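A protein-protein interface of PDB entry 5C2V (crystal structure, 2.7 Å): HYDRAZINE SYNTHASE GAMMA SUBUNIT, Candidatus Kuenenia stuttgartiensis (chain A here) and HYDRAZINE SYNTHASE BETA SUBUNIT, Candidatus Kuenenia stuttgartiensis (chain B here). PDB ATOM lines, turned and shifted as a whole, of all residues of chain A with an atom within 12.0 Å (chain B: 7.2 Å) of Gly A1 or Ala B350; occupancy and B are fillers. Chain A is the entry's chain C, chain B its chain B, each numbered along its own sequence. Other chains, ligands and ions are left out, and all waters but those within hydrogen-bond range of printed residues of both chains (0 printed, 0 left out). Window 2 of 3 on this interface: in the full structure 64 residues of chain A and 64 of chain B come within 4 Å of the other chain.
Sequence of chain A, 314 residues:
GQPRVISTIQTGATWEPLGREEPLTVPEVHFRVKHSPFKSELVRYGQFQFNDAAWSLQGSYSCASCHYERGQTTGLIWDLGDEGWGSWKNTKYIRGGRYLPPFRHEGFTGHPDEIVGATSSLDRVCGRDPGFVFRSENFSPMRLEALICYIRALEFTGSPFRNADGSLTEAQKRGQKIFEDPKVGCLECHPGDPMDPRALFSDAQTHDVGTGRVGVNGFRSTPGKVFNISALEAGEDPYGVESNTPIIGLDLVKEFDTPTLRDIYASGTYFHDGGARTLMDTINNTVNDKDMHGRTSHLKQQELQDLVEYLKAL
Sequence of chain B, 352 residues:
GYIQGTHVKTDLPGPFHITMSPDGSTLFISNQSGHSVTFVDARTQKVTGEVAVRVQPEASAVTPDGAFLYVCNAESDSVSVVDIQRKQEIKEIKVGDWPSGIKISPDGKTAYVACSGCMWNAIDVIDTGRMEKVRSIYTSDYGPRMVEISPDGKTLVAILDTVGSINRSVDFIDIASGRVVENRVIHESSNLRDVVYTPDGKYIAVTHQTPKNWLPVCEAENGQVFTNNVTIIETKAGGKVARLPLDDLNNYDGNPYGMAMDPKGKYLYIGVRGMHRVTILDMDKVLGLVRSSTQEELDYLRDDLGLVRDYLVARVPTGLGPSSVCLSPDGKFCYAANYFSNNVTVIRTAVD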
ATOM      1  N   GLY A   1      21.286  11.112   6.858  1.00  0.00           N
ATOM      2  CA  GLY A   1      21.134   9.777   7.407  1.00  0.00           C
ATOM      3  C   GLY A   1      19.985   9.684   8.391  1.00  0.00           C
ATOM      4  O   GLY A   1      19.127  10.564   8.441  1.00  0.00           O
ATOM      5  N   GLN A   2      19.967   8.612   9.175  1.00  0.00           N
ATOM      6  CA  GLN A   2      18.923   8.416  10.174  1.00  0.00           C
ATOM      7  C   GLN A   2      19.366   8.942  11.538  1.00  0.00           C
ATOM      8  O   GLN A   2      20.452   8.610  12.016  1.00  0.00           O
ATOM      9  CB  GLN A   2      18.530   6.935  10.270  1.00  0.00           C
ATOM     10  CG  GLN A   2      19.685   5.969  10.528  1.00  0.00           C
ATOM     11  CD  GLN A   2      20.452   5.607   9.268  1.00  0.00           C
ATOM     12  OE1 GLN A   2      20.234   6.187   8.203  1.00  0.00           O
ATOM     13  NE2 GLN A   2      21.356   4.641   9.384  1.00  0.00           N
ATOM     14  N   PRO A   3      18.527   9.786  12.160  1.00  0.00           N
ATOM     15  CA  PRO A   3      18.800  10.369  13.479  1.00  0.00           C
ATOM     16  C   PRO A   3      19.017   9.307  14.555  1.00  0.00           C
ATOM     17  O   PRO A   3      18.231   8.365  14.656  1.00  0.00           O
ATOM     18  CB  PRO A   3      17.540  11.188  13.766  1.00  0.00           C
ATOM     19  CG  PRO A   3      16.996  11.517  12.419  1.00  0.00           C
ATOM     20  CD  PRO A   3      17.281  10.311  11.575  1.00  0.00           C
ATOM     21  N   ARG A   4      20.072   9.467  15.349  1.00  0.00           N
ATOM     22  CA  ARG A   4      20.426   8.474  16.357  1.00  0.00           C
ATOM     23  C   ARG A   4      21.171   9.097  17.537  1.00  0.00           C
ATOM     24  O   ARG A   4      21.691  10.208  17.436  1.00  0.00           O
ATOM     25  CB  ARG A   4      21.279   7.369  15.731  1.00  0.00           C
ATOM     26  CG  ARG A   4      22.684   7.816  15.353  1.00  0.00           C
ATOM     27  CD  ARG A   4      23.407   6.755  14.539  1.00  0.00           C
ATOM     28  NE  ARG A   4      24.848   6.989  14.490  1.00  0.00           N
ATOM     29  CZ  ARG A   4      25.444   7.825  13.646  1.00  0.00           C
ATOM     30  NH1 ARG A   4      24.724   8.519  12.774  1.00  0.00           N
ATOM     31  NH2 ARG A   4      26.762   7.971  13.675  1.00  0.00           N
ATOM     32  N   VAL A   5      21.223   8.372  18.653  1.00  0.00           N
ATOM     33  CA  VAL A   5      21.945   8.833  19.835  1.00  0.00           C
ATOM     34  C   VAL A   5      23.374   8.307  19.845  1.00  0.00           C
ATOM     35  O   VAL A   5      23.604   7.106  19.999  1.00  0.00           O
ATOM     36  CB  VAL A   5      21.252   8.392  21.142  1.00  0.00           C
ATOM     37  CG1 VAL A   5      22.150   8.669  22.341  1.00  0.00           C
ATOM     38  CG2 VAL A   5      19.920   9.091  21.303  1.00  0.00           C
ATOM     39  N   ILE A   6      24.332   9.211  19.668  1.00  0.00           N
ATOM     40  CA  ILE A   6      25.742   8.850  19.731  1.00  0.00           C
ATOM     41  C   ILE A   6      26.289   8.809  21.163  1.00  0.00           C
ATOM     42  O   ILE A   6      27.073   7.922  21.502  1.00  0.00           O
ATOM     43  CB  ILE A   6      26.603   9.814  18.886  1.00  0.00           C
ATOM     44  CG1 ILE A   6      26.309  11.269  19.252  1.00  0.00           C
ATOM     45  CG2 ILE A   6      26.351   9.586  17.402  1.00  0.00           C
ATOM     46  CD1 ILE A   6      27.105  12.266  18.449  1.00  0.00           C
ATOM     47  N   TYR B 267      14.191  20.756   9.331  1.00  0.00           N
ATOM     48  CA  TYR B 267      13.588  19.896  10.344  1.00  0.00           C
ATOM     49  C   TYR B 267      13.118  20.665  11.572  1.00  0.00           C
ATOM     50  O   TYR B 267      13.616  21.751  11.868  1.00  0.00           O
ATOM     51  CB  TYR B 267      14.578  18.814  10.782  1.00  0.00           C
ATOM     52  CG  TYR B 267      15.044  17.907   9.669  1.00  0.00           C
ATOM     53  CD1 TYR B 267      14.316  16.780   9.315  1.00  0.00           C
ATOM     54  CD2 TYR B 267      16.219  18.172   8.979  1.00  0.00           C
ATOM     55  CE1 TYR B 267      14.740  15.944   8.300  1.00  0.00           C
ATOM     56  CE2 TYR B 267      16.651  17.344   7.962  1.00  0.00           C
ATOM     57  CZ  TYR B 267      15.908  16.231   7.627  1.00  0.00           C
ATOM     58  OH  TYR B 267      16.334  15.402   6.615  1.00  0.00           O
ATOM     59  N   TYR B 269      12.579  20.089  15.785  1.00  0.00           N
ATOM     60  CA  TYR B 269      12.930  19.209  16.895  1.00  0.00           C
ATOM     61  C   TYR B 269      12.100  19.538  18.130  1.00  0.00           C
ATOM     62  O   TYR B 269      12.062  20.683  18.571  1.00  0.00           O
ATOM     63  CB  TYR B 269      14.425  19.318  17.208  1.00  0.00           C
ATOM     64  CG  TYR B 269      15.312  18.999  16.024  1.00  0.00           C
ATOM     65  CD1 TYR B 269      15.613  19.968  15.076  1.00  0.00           C
ATOM     66  CD2 TYR B 269      15.842  17.728  15.852  1.00  0.00           C
ATOM     67  CE1 TYR B 269      16.415  19.681  13.990  1.00  0.00           C
ATOM     68  CE2 TYR B 269      16.651  17.432  14.768  1.00  0.00           C
ATOM     69  CZ  TYR B 269      16.933  18.414  13.842  1.00  0.00           C
ATOM     70  OH  TYR B 269      17.734  18.133  12.760  1.00  0.00           O
ATOM     71  N   ILE B 280      11.358  14.370  15.867  1.00  0.00           N
ATOM     72  CA  ILE B 280      11.901  15.113  14.739  1.00  0.00           C
ATOM     73  C   ILE B 280      10.967  15.030  13.539  1.00  0.00           C
ATOM     74  O   ILE B 280      10.609  13.933  13.090  1.00  0.00           O
ATOM     75  CB  ILE B 280      13.291  14.594  14.337  1.00  0.00           C
ATOM     76  CG1 ILE B 280      14.184  14.454  15.572  1.00  0.00           C
ATOM     77  CG2 ILE B 280      13.926  15.513  13.303  1.00  0.00           C
ATOM     78  CD1 ILE B 280      15.541  13.859  15.279  1.00  0.00           C
ATOM     79  N   VAL B 313       9.750  12.379  10.806  1.00  0.00           N
ATOM     80  CA  VAL B 313      11.077  11.839  10.535  1.00  0.00           C
ATOM     81  C   VAL B 313      11.481  10.758  11.532  1.00  0.00           C
ATOM     82  O   VAL B 313      11.815   9.639  11.141  1.00  0.00           O
ATOM     83  CB  VAL B 313      12.150  12.946  10.545  1.00  0.00           C
ATOM     84  CG1 VAL B 313      13.531  12.348  10.313  1.00  0.00           C
ATOM     85  CG2 VAL B 313      11.835  14.002   9.498  1.00  0.00           C
ATOM     86  N   GLY B 331      23.598  22.506  12.450  1.00  0.00           N
ATOM     87  CA  GLY B 331      22.387  21.706  12.477  1.00  0.00           C
ATOM     88  C   GLY B 331      22.596  20.204  12.419  1.00  0.00           C
ATOM     89  O   GLY B 331      21.644  19.451  12.212  1.00  0.00           O
ATOM     90  N   LYS B 332      23.834  19.760  12.605  1.00  0.00           N
ATOM     91  CA  LYS B 332      24.138  18.333  12.535  1.00  0.00           C
ATOM     92  C   LYS B 332      24.031  17.637  13.891  1.00  0.00           C
ATOM     93  O   LYS B 332      24.131  16.413  13.973  1.00  0.00           O
ATOM     94  CB  LYS B 332      25.532  18.117  11.938  1.00  0.00           C
ATOM     95  CG  LYS B 332      25.974  19.223  10.997  1.00  0.00           C
ATOM     96  CD  LYS B 332      26.957  18.713   9.952  1.00  0.00           C
ATOM     97  CE  LYS B 332      28.147  18.017  10.591  1.00  0.00           C
ATOM     98  NZ  LYS B 332      29.114  17.529   9.568  1.00  0.00           N
ATOM     99  N   ILE B 347      22.340  13.980  20.007  1.00  0.00           N
ATOM    100  CA  ILE B 347      21.734  13.305  18.867  1.00  0.00           C
ATOM    101  C   ILE B 347      22.357  13.746  17.547  1.00  0.00           C
ATOM    102  O   ILE B 347      22.495  14.939  17.284  1.00  0.00           O
ATOM    103  CB  ILE B 347      20.214  13.567  18.804  1.00  0.00           C
ATOM    104  CG1 ILE B 347      19.583  13.427  20.191  1.00  0.00           C
ATOM    105  CG2 ILE B 347      19.548  12.639  17.800  1.00  0.00           C
ATOM    106  CD1 ILE B 347      18.114  13.790  20.230  1.00  0.00           C
ATOM    107  N   ARG B 348      22.731  12.776  16.718  1.00  0.00           N
ATOM    108  CA  ARG B 348      23.191  13.067  15.366  1.00  0.00           C
ATOM    109  C   ARG B 348      21.980  13.157  14.447  1.00  0.00           C
ATOM    110  O   ARG B 348      21.234  12.191  14.301  1.00  0.00           O
ATOM    111  CB  ARG B 348      24.163  11.991  14.877  1.00  0.00           C
ATOM    112  CG  ARG B 348      24.665  12.191  13.454  1.00  0.00           C
ATOM    113  CD  ARG B 348      25.559  13.414  13.343  1.00  0.00           C
ATOM    114  NE  ARG B 348      26.219  13.493  12.044  1.00  0.00           N
ATOM    115  CZ  ARG B 348      25.772  14.212  11.019  1.00  0.00           C
ATOM    116  NH1 ARG B 348      24.660  14.923  11.141  1.00  0.00           N
ATOM    117  NH2 ARG B 348      26.439  14.223   9.873  1.00  0.00           N
ATOM    118  N   THR B 349      21.783  14.317  13.832  1.00  0.00           N
ATOM    119  CA  THR B 349      20.588  14.557  13.032  1.00  0.00           C
ATOM    120  C   THR B 349      20.708  13.977  11.627  1.00  0.00           C
ATOM    121  O   THR B 349      21.722  13.373  11.275  1.00  0.00           O
ATOM    122  CB  THR B 349      20.279  16.060  12.926  1.00  0.00           C
ATOM    123  OG1 THR B 349      21.322  16.715  12.194  1.00  0.00           O
ATOM    124  CG2 THR B 349      20.172  16.678  14.313  1.00  0.00           C
ATOM    125  N   ALA B 350      19.661  14.166  10.829  1.00  0.00           N
ATOM    126  CA  ALA B 350      19.630  13.662   9.461  1.00  0.00           C
ATOM    127  C   ALA B 350      20.535  14.483   8.550  1.00  0.00           C
ATOM    128  O   ALA B 350      20.943  14.020   7.484  1.00  0.00           O
ATOM    129  CB  ALA B 350      18.205  13.661   8.931  1.00  0.00           C
ATOM    130  N   VAL B 351      20.839  15.705   8.976  1.00  0.00           N
ATOM    131  CA  VAL B 351      21.691  16.604   8.205  1.00  0.00           C
ATOM    132  C   VAL B 351      23.102  16.039   8.062  1.00  0.00           C
ATOM    133  O   VAL B 351      23.704  15.592   9.037  1.00  0.00           O
ATOM    134  CB  VAL B 351      21.766  18.000   8.853  1.00  0.00           C
ATOM    135  CG1 VAL B 351      22.574  18.950   7.984  1.00  0.00           C
ATOM    136  CG2 VAL B 351      20.367  18.549   9.089  1.00  0.00           C
ATOM    137  N   ASP B 352      23.620  16.056   6.838  1.00  0.00           N
ATOM    138  CA  ASP B 352      24.957  15.545   6.564  1.00  0.00           C
ATOM    139  C   ASP B 352      25.724  16.478   5.632  1.00  0.00           C
ATOM    140  O   ASP B 352      25.808  17.682   5.874  1.00  0.00           O
ATOM    141  CB  ASP B 352      24.879  14.143   5.957  1.00  0.00           C
ATOM    142  CG  ASP B 352      23.974  14.084   4.742  1.00  0.00           C
ATOM    143  OD1 ASP B 352      23.093  14.959   4.612  1.00  0.00           O
ATOM    144  OD2 ASP B 352      24.143  13.160   3.918  1.00  0.00           O
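The backbone carbonyl oxygen (O) of Arg A4 lies within hydrogen-bond range of the backbone NH (N) of Arg B348.
The backbone NH of Gly A1 sits at hydrogen-bond distance from the backbone carbonyl oxygen of Ala B350 (3.0 Å).
O of Ile B280 is in hydrogen-bond range of N of Val B313 (2.9 Å).
O of Lys B332 lies within hydrogen-bond range of NH1 of Arg B348 (3.2 Å).
The backbone carbonyl oxygen (O) of Val B351 sits at hydrogen-bond distance from the guanidinium group (NH1) of Arg B348, at 2.4 Å.
Ile B280 touches Pro A3.
CA of Pro A3 touches O of Arg B348, at 3.1 Å.
CG2 of Ile B347 touches O of Arg A4 (3.3 Å).
Gly A1 touches just one residue of chain B: Ala B350.
Ala B350 touches just one residue of chain A: Gly A1.
Of chain A, only Pro A3 (3.1 Å) and Arg A4 (2.9 Å) come within 4 Å of Arg B348.
No residue of chain A comes within 4 Å of Thr B349.
No residue of chain A comes within 4 Å of Asp B352.
Printed residues of chain B within 4 Å of Pro A3: Ile B280 (3.7 Å) and Arg B348 (3.1 Å).
Of the printed residues of chain B, Arg A4 touches Ile B347 (3.3 Å) and Arg B348 (2.9 Å).
Tyr B269 touches none of the printed residues of chain A.
Gly B331 touches none of the printed residues of chain A.
The nearest residue of chain B that does not touch Gly A1 is Asp B352 (4.5 Å).
The nearest residue of chain A that does not touch Ala B350 is Pro A3 (4.1 Å).
Of the 6 printed residues of chain A, 3 touch a printed residue of chain B.
Hydrophobic or aromatic side chains of chain A that line the printed part of chain B: Pro A3.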
